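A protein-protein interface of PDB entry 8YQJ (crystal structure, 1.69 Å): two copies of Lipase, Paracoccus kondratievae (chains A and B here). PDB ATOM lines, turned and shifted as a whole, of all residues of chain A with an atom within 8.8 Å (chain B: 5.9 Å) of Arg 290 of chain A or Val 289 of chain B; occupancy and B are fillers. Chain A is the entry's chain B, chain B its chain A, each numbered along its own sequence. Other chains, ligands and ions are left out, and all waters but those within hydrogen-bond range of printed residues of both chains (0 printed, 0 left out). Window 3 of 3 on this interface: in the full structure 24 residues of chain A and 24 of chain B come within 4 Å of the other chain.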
ATOM      1  N   VAL A  70       9.166  10.036  -1.773  1.00  0.00           N
ATOM      2  CA  VAL A  70       9.590  11.283  -1.146  1.00  0.00           C
ATOM      3  C   VAL A  70      10.877  10.999  -0.389  1.00  0.00           C
ATOM      4  O   VAL A  70      11.020   9.937   0.227  1.00  0.00           O
ATOM      5  CB  VAL A  70       8.515  11.841  -0.188  1.00  0.00           C
ATOM      6  CG1 VAL A  70       9.018  13.065   0.552  1.00  0.00           C
ATOM      7  CG2 VAL A  70       7.235  12.152  -0.945  1.00  0.00           C
ATOM      8  N   PRO A 133      10.877  14.837  -5.011  1.00  0.00           N
ATOM      9  CA  PRO A 133      10.207  15.486  -3.880  1.00  0.00           C
ATOM     10  C   PRO A 133      10.962  15.162  -2.603  1.00  0.00           C
ATOM     11  O   PRO A 133      11.347  14.013  -2.382  1.00  0.00           O
ATOM     12  CB  PRO A 133       8.816  14.847  -3.890  1.00  0.00           C
ATOM     13  CG  PRO A 133       8.576  14.582  -5.345  1.00  0.00           C
ATOM     14  CD  PRO A 133       9.926  14.020  -5.787  1.00  0.00           C
ATOM     15  N   VAL A 135      11.598  16.490   1.751  1.00  0.00           N
ATOM     16  CA  VAL A 135      11.660  17.377   2.907  1.00  0.00           C
ATOM     17  C   VAL A 135      13.127  17.689   3.178  1.00  0.00           C
ATOM     18  O   VAL A 135      14.004  16.850   2.967  1.00  0.00           O
ATOM     19  CB  VAL A 135      10.996  16.709   4.128  1.00  0.00           C
ATOM     20  CG1 VAL A 135      11.009  17.636   5.316  1.00  0.00           C
ATOM     21  CG2 VAL A 135       9.589  16.219   3.798  1.00  0.00           C
ATOM     22  N   LEU A 160       9.326  20.033   0.142  1.00  0.00           N
ATOM     23  CA  LEU A 160       7.983  19.834   0.657  1.00  0.00           C
ATOM     24  C   LEU A 160       7.792  20.475   2.020  1.00  0.00           C
ATOM     25  O   LEU A 160       6.650  20.755   2.408  1.00  0.00           O
ATOM     26  CB  LEU A 160       7.648  18.349   0.733  1.00  0.00           C
ATOM     27  CG  LEU A 160       7.900  17.545  -0.530  1.00  0.00           C
ATOM     28  CD1 LEU A 160       7.575  16.086  -0.271  1.00  0.00           C
ATOM     29  CD2 LEU A 160       6.996  18.099  -1.616  1.00  0.00           C
ATOM     30  N   GLY A 161       8.880  20.722   2.726  1.00  0.00           N
ATOM     31  CA  GLY A 161       8.828  21.302   4.051  1.00  0.00           C
ATOM     32  C   GLY A 161      10.247  21.467   4.540  1.00  0.00           C
ATOM     33  O   GLY A 161      11.181  20.853   4.018  1.00  0.00           O
ATOM     34  N   PRO A 222       6.727  25.203   3.770  1.00  0.00           N
ATOM     35  CA  PRO A 222       6.186  25.256   5.132  1.00  0.00           C
ATOM     36  C   PRO A 222       7.211  24.708   6.109  1.00  0.00           C
ATOM     37  O   PRO A 222       8.053  23.880   5.758  1.00  0.00           O
ATOM     38  CB  PRO A 222       4.932  24.374   5.063  1.00  0.00           C
ATOM     39  CG  PRO A 222       5.097  23.538   3.819  1.00  0.00           C
ATOM     40  CD  PRO A 222       5.875  24.405   2.868  1.00  0.00           C
ATOM     41  N   ALA A 223       7.135  25.178   7.344  1.00  0.00           N
ATOM     42  CA  ALA A 223       8.238  25.015   8.279  1.00  0.00           C
ATOM     43  C   ALA A 223       7.760  24.494   9.623  1.00  0.00           C
ATOM     44  O   ALA A 223       6.729  24.919  10.143  1.00  0.00           O
ATOM     45  CB  ALA A 223       8.971  26.331   8.494  1.00  0.00           C
ATOM     46  N   ALA A 250       2.960  28.631   6.111  1.00  0.00           N
ATOM     47  CA  ALA A 250       2.558  27.807   7.239  1.00  0.00           C
ATOM     48  C   ALA A 250       3.788  27.419   8.027  1.00  0.00           C
ATOM     49  O   ALA A 250       4.725  26.821   7.481  1.00  0.00           O
ATOM     50  CB  ALA A 250       1.822  26.554   6.777  1.00  0.00           C
ATOM     51  N   ALA A 251       3.795  27.767   9.305  1.00  0.00           N
ATOM     52  CA  ALA A 251       4.972  27.519  10.120  1.00  0.00           C
ATOM     53  C   ALA A 251       4.533  27.329  11.556  1.00  0.00           C
ATOM     54  O   ALA A 251       3.622  28.013  12.039  1.00  0.00           O
ATOM     55  CB  ALA A 251       5.987  28.657  10.027  1.00  0.00           C
ATOM     56  N   GLU A 252       5.178  26.385  12.219  1.00  0.00           N
ATOM     57  CA  GLU A 252       4.919  26.093  13.615  1.00  0.00           C
ATOM     58  C   GLU A 252       6.214  26.239  14.412  1.00  0.00           C
ATOM     59  O   GLU A 252       7.282  25.777  13.985  1.00  0.00           O
ATOM     60  CB  GLU A 252       4.333  24.695  13.767  1.00  0.00           C
ATOM     61  CG  GLU A 252       4.074  24.311  15.193  1.00  0.00           C
ATOM     62  CD  GLU A 252       3.310  23.022  15.298  1.00  0.00           C
ATOM     63  OE1 GLU A 252       3.556  22.118  14.475  1.00  0.00           O
ATOM     64  OE2 GLU A 252       2.453  22.914  16.209  1.00  0.00           O
ATOM     65  N   SER A 282       7.597  13.164  13.487  1.00  0.00           N
ATOM     66  CA  SER A 282       6.218  13.378  13.055  1.00  0.00           C
ATOM     67  C   SER A 282       6.125  14.538  12.079  1.00  0.00           C
ATOM     68  O   SER A 282       5.376  14.474  11.102  1.00  0.00           O
ATOM     69  CB  SER A 282       5.301  13.637  14.260  1.00  0.00           C
ATOM     70  OG  SER A 282       5.349  12.550  15.175  1.00  0.00           O
ATOM     71  N   ALA A 283       6.886  15.608  12.322  1.00  0.00           N
ATOM     72  CA  ALA A 283       6.810  16.763  11.437  1.00  0.00           C
ATOM     73  C   ALA A 283       7.389  16.425  10.078  1.00  0.00           C
ATOM     74  O   ALA A 283       6.866  16.859   9.043  1.00  0.00           O
ATOM     75  CB  ALA A 283       7.551  17.953  12.052  1.00  0.00           C
ATOM     76  N   ILE A 284       8.472  15.649  10.067  1.00  0.00           N
ATOM     77  CA  ILE A 284       9.040  15.226   8.795  1.00  0.00           C
ATOM     78  C   ILE A 284       8.042  14.365   8.047  1.00  0.00           C
ATOM     79  O   ILE A 284       7.806  14.550   6.843  1.00  0.00           O
ATOM     80  CB  ILE A 284      10.359  14.479   9.023  1.00  0.00           C
ATOM     81  CG1 ILE A 284      11.439  15.432   9.506  1.00  0.00           C
ATOM     82  CG2 ILE A 284      10.817  13.812   7.714  1.00  0.00           C
ATOM     83  CD1 ILE A 284      12.680  14.698   9.925  1.00  0.00           C
ATOM     84  N   MET A 285       7.411  13.431   8.762  1.00  0.00           N
ATOM     85  CA  MET A 285       6.451  12.537   8.133  1.00  0.00           C
ATOM     86  C   MET A 285       5.285  13.352   7.573  1.00  0.00           C
ATOM     87  O   MET A 285       4.826  13.125   6.450  1.00  0.00           O
ATOM     88  CB  MET A 285       5.903  11.556   9.165  1.00  0.00           C
ATOM     89  CG  MET A 285       5.286  10.239   8.652  1.00  0.00           C
ATOM     90  SD  MET A 285       6.241   9.314   7.388  1.00  0.00           S
ATOM     91  CE  MET A 285       5.879  10.098   5.825  1.00  0.00           C
ATOM     92  N   ARG A 286       4.778  14.304   8.378  1.00  0.00           N
ATOM     93  CA  ARG A 286       3.687  15.191   7.983  1.00  0.00           C
ATOM     94  C   ARG A 286       3.983  15.891   6.667  1.00  0.00           C
ATOM     95  O   ARG A 286       3.168  15.878   5.739  1.00  0.00           O
ATOM     96  CB  ARG A 286       3.466  16.248   9.077  1.00  0.00           C
ATOM     97  CG  ARG A 286       2.186  17.065   8.990  1.00  0.00           C
ATOM     98  CD  ARG A 286       1.686  17.362  10.404  1.00  0.00           C
ATOM     99  NE  ARG A 286       2.700  18.027  11.220  1.00  0.00           N
ATOM    100  CZ  ARG A 286       2.937  17.754  12.499  1.00  0.00           C
ATOM    101  NH1 ARG A 286       2.279  16.799  13.139  1.00  0.00           N
ATOM    102  NH2 ARG A 286       3.868  18.444  13.151  1.00  0.00           N
ATOM    103  N   PHE A 287       5.135  16.560   6.593  1.00  0.00           N
ATOM    104  CA  PHE A 287       5.493  17.262   5.367  1.00  0.00           C
ATOM    105  C   PHE A 287       5.658  16.301   4.204  1.00  0.00           C
ATOM    106  O   PHE A 287       5.365  16.651   3.056  1.00  0.00           O
ATOM    107  CB  PHE A 287       6.785  18.048   5.549  1.00  0.00           C
ATOM    108  CG  PHE A 287       6.635  19.266   6.401  1.00  0.00           C
ATOM    109  CD1 PHE A 287       5.525  20.078   6.286  1.00  0.00           C
ATOM    110  CD2 PHE A 287       7.630  19.618   7.283  1.00  0.00           C
ATOM    111  CE1 PHE A 287       5.397  21.223   7.085  1.00  0.00           C
ATOM    112  CE2 PHE A 287       7.526  20.747   8.068  1.00  0.00           C
ATOM    113  CZ  PHE A 287       6.399  21.558   7.967  1.00  0.00           C
ATOM    114  N   ALA A 288       6.178  15.101   4.473  1.00  0.00           N
ATOM    115  CA  ALA A 288       6.409  14.148   3.396  1.00  0.00           C
ATOM    116  C   ALA A 288       5.093  13.654   2.812  1.00  0.00           C
ATOM    117  O   ALA A 288       4.959  13.541   1.587  1.00  0.00           O
ATOM    118  CB  ALA A 288       7.248  12.975   3.892  1.00  0.00           C
ATOM    119  N   VAL A 289       4.108  13.369   3.671  1.00  0.00           N
ATOM    120  CA  VAL A 289       2.819  12.878   3.194  1.00  0.00           C
ATOM    121  C   VAL A 289       2.063  13.966   2.449  1.00  0.00           C
ATOM    122  O   VAL A 289       1.481  13.716   1.388  1.00  0.00           O
ATOM    123  CB  VAL A 289       1.983  12.322   4.359  1.00  0.00           C
ATOM    124  CG1 VAL A 289       0.603  11.932   3.872  1.00  0.00           C
ATOM    125  CG2 VAL A 289       2.683  11.113   4.968  1.00  0.00           C
ATOM    126  N   ARG A 290       2.063  15.193   2.979  1.00  0.00           N
ATOM    127  CA  ARG A 290       1.328  16.296   2.363  1.00  0.00           C
ATOM    128  C   ARG A 290       1.880  16.643   0.978  1.00  0.00           C
ATOM    129  O   ARG A 290       1.520  17.673   0.403  1.00  0.00           O
ATOM    130  CB  ARG A 290       1.359  17.533   3.271  1.00  0.00           C
ATOM    131  CG  ARG A 290       0.256  17.570   4.340  1.00  0.00           C
ATOM    132  CD  ARG A 290       0.540  18.602   5.444  1.00  0.00           C
ATOM    133  NE  ARG A 290      -0.093  18.252   6.715  1.00  0.00           N
ATOM    134  CZ  ARG A 290      -0.349  19.109   7.699  1.00  0.00           C
ATOM    135  NH1 ARG A 290      -0.072  20.399   7.585  1.00  0.00           N
ATOM    136  NH2 ARG A 290      -0.892  18.659   8.828  1.00  0.00           N
ATOM    137  N   GLY A 291       2.744  15.796   0.429  1.00  0.00           N
ATOM    138  CA  GLY A 291       3.293  16.021  -0.893  1.00  0.00           C
ATOM    139  C   GLY A 291       3.067  14.844  -1.813  1.00  0.00           C
ATOM    140  O   GLY A 291       3.582  13.751  -1.570  1.00  0.00           O
ATOM    141  N   VAL B  70      -7.928  15.820  13.282  1.00  0.00           N
ATOM    142  CA  VAL B  70      -7.822  14.369  13.322  1.00  0.00           C
ATOM    143  C   VAL B  70      -7.348  13.988  14.711  1.00  0.00           C
ATOM    144  O   VAL B  70      -6.469  14.643  15.272  1.00  0.00           O
ATOM    145  CB  VAL B  70      -6.853  13.827  12.258  1.00  0.00           C
ATOM    146  CG1 VAL B  70      -6.671  12.302  12.406  1.00  0.00           C
ATOM    147  CG2 VAL B  70      -7.371  14.176  10.879  1.00  0.00           C
ATOM    148  N   ILE B 284       1.211   6.643  12.668  1.00  0.00           N
ATOM    149  CA  ILE B 284       0.016   7.354  13.114  1.00  0.00           C
ATOM    150  C   ILE B 284      -0.114   8.688  12.388  1.00  0.00           C
ATOM    151  O   ILE B 284      -1.190   9.046  11.882  1.00  0.00           O
ATOM    152  CB  ILE B 284       0.081   7.562  14.631  1.00  0.00           C
ATOM    153  CG1 ILE B 284      -0.089   6.231  15.362  1.00  0.00           C
ATOM    154  CG2 ILE B 284      -0.974   8.594  15.086  1.00  0.00           C
ATOM    155  CD1 ILE B 284       0.113   6.340  16.885  1.00  0.00           C
ATOM    156  N   MET B 285       0.971   9.470  12.381  1.00  0.00           N
ATOM    157  CA  MET B 285       1.003  10.720  11.627  1.00  0.00           C
ATOM    158  C   MET B 285       0.653  10.497  10.157  1.00  0.00           C
ATOM    159  O   MET B 285      -0.102  11.273   9.563  1.00  0.00           O
ATOM    160  CB  MET B 285       2.385  11.362  11.760  1.00  0.00           C
ATOM    161  CG  MET B 285       2.392  12.822  11.408  1.00  0.00           C
ATOM    162  SD  MET B 285       1.671  13.778  12.760  1.00  0.00           S
ATOM    163  CE  MET B 285       0.285  14.519  11.899  1.00  0.00           C
ATOM    164  N   ARG B 286       1.205   9.440   9.550  1.00  0.00           N
ATOM    165  CA  ARG B 286       0.965   9.176   8.139  1.00  0.00           C
ATOM    166  C   ARG B 286      -0.523   8.935   7.878  1.00  0.00           C
ATOM    167  O   ARG B 286      -1.100   9.489   6.937  1.00  0.00           O
ATOM    168  CB  ARG B 286       1.783   7.957   7.705  1.00  0.00           C
ATOM    169  CG  ARG B 286       1.629   7.554   6.265  1.00  0.00           C
ATOM    170  CD  ARG B 286       2.800   6.645   5.846  1.00  0.00           C
ATOM    171  NE  ARG B 286       3.314   5.887   6.989  1.00  0.00           N
ATOM    172  CZ  ARG B 286       4.517   5.326   7.071  1.00  0.00           C
ATOM    173  NH1 ARG B 286       5.414   5.460   6.106  1.00  0.00           N
ATOM    174  NH2 ARG B 286       4.817   4.590   8.138  1.00  0.00           N
ATOM    175  N   PHE B 287      -1.169   8.125   8.723  1.00  0.00           N
ATOM    176  CA  PHE B 287      -2.593   7.866   8.531  1.00  0.00           C
ATOM    177  C   PHE B 287      -3.424   9.118   8.764  1.00  0.00           C
ATOM    178  O   PHE B 287      -4.418   9.352   8.060  1.00  0.00           O
ATOM    179  CB  PHE B 287      -3.077   6.757   9.463  1.00  0.00           C
ATOM    180  CG  PHE B 287      -2.627   5.390   9.077  1.00  0.00           C
ATOM    181  CD1 PHE B 287      -2.614   4.990   7.742  1.00  0.00           C
ATOM    182  CD2 PHE B 287      -2.247   4.484  10.057  1.00  0.00           C
ATOM    183  CE1 PHE B 287      -2.204   3.704   7.393  1.00  0.00           C
ATOM    184  CE2 PHE B 287      -1.850   3.208   9.716  1.00  0.00           C
ATOM    185  CZ  PHE B 287      -1.838   2.814   8.384  1.00  0.00           C
ATOM    186  N   ALA B 288      -3.054   9.913   9.761  1.00  0.00           N
ATOM    187  CA  ALA B 288      -3.807  11.124  10.053  1.00  0.00           C
ATOM    188  C   ALA B 288      -3.727  12.109   8.901  1.00  0.00           C
ATOM    189  O   ALA B 288      -4.711  12.786   8.586  1.00  0.00           O
ATOM    190  CB  ALA B 288      -3.285  11.777  11.335  1.00  0.00           C
ATOM    191  N   VAL B 289      -2.561  12.219   8.266  1.00  0.00           N
ATOM    192  CA  VAL B 289      -2.419  13.247   7.244  1.00  0.00           C
ATOM    193  C   VAL B 289      -3.056  12.794   5.939  1.00  0.00           C
ATOM    194  O   VAL B 289      -3.702  13.589   5.244  1.00  0.00           O
ATOM    195  CB  VAL B 289      -0.939  13.626   7.062  1.00  0.00           C
ATOM    196  CG1 VAL B 289      -0.790  14.598   5.904  1.00  0.00           C
ATOM    197  CG2 VAL B 289      -0.406  14.273   8.349  1.00  0.00           C
ATOM    198  N   ARG B 290      -2.895  11.517   5.583  1.00  0.00           N
ATOM    199  CA  ARG B 290      -3.608  10.994   4.423  1.00  0.00           C
ATOM    200  C   ARG B 290      -5.106  11.247   4.556  1.00  0.00           C
ATOM    201  O   ARG B 290      -5.738  11.823   3.664  1.00  0.00           O
ATOM    202  CB  ARG B 290      -3.351   9.500   4.274  1.00  0.00           C
ATOM    203  CG  ARG B 290      -1.928   9.074   4.044  1.00  0.00           C
ATOM    204  CD  ARG B 290      -1.845   8.044   2.948  1.00  0.00           C
ATOM    205  NE  ARG B 290      -0.455   7.753   2.626  1.00  0.00           N
ATOM    206  CZ  ARG B 290       0.258   6.793   3.207  1.00  0.00           C
ATOM    207  NH1 ARG B 290      -0.274   5.977   4.112  1.00  0.00           N
ATOM    208  NH2 ARG B 290       1.532   6.639   2.868  1.00  0.00           N
ATOM    209  N   GLY B 291      -5.687  10.836   5.680  1.00  0.00           N
ATOM    210  CA  GLY B 291      -7.110  11.016   5.914  1.00  0.00           C
ATOM    211  C   GLY B 291      -7.635  12.439   5.829  1.00  0.00           C
ATOM    212  O   GLY B 291      -7.325  13.287   6.671  1.00  0.00           O
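Among the printed residues, merely in contact across the chains: Ser 282 of chain A with Met 285 of chain B, Arg 290 of chain A with Val 289 of chain B, Val 289 of chain A with Val 289 of chain B, Val 289 of chain A with Arg 290 of chain B, Arg 286 of chain A with Val 289 of chain B and Val 289 of chain A with Arg 286 of chain B.
The side-chain sulfur (SD) of Met 285 of chain B lies within hydrogen-bond range of the guanidinium group (NH1) of Arg 286 of chain A, at 3.1 Å.
Arg 286 of chain A touches Met 285 of chain B, but with the chains exchanged Met 285 of chain A does not touch Arg 286 of chain B (4.1 Å).
Arg 286 of chain A touches Val 289 of chain B, and with the chains exchanged Val 289 of chain A touches Arg 286 of chain B.
Val 289 of chain B touches its own counterpart, Val 289 of chain A.
Val 289 of chain A touches Arg 290 of chain B, and with the chains exchanged Arg 290 of chain A touches Val 289 of chain B.
9 positions are printed for both chains.
Of the 7 pairs that touch across the chains among the printed residues, 5 have their exchanged pair printed and touching as well.
Printed residues of chain B that touch a printed residue of chain A: Met 285, Arg 286, Val 289 and Arg 290.
Hydrophobic or aromatic side chains of chain B that line the printed part of chain A: Met 285 and Val 289.
Hydrophobic or aromatic side chains of chain A that line the printed part of chain B: Val 289.
Among the printed residues, no Asp or Glu carboxylate lies within 4 Å of a Lys or Arg side-chain nitrogen of the other chain.
OE1 of Glu 252 of chain A lies within salt-bridge range of NH2 of Arg 286 of chain A (3.9 Å).
Of the printed residues of chain B, Ser 282 of chain A touches Met 285.
Arg 290 of chain A touches just one residue of chain B: Val 289 (3.5 Å).
Phe 287 of chain B touches none of the printed residues of chain A.
No residue of chain A comes within 4 Å of Ala 288 of chain B.
Of the printed residues of chain A, Arg 290 of chain B touches Val 289 (3.8 Å).
No residue of chain A comes within 4 Å of Gly 291 of chain B.
The nearest residue of chain B that does not touch Arg 290 of chain A is Met 285 of chain B (5.3 Å).
The nearest residue of chain A that does not touch Val 289 of chain B is Met 285 of chain A (5.7 Å).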
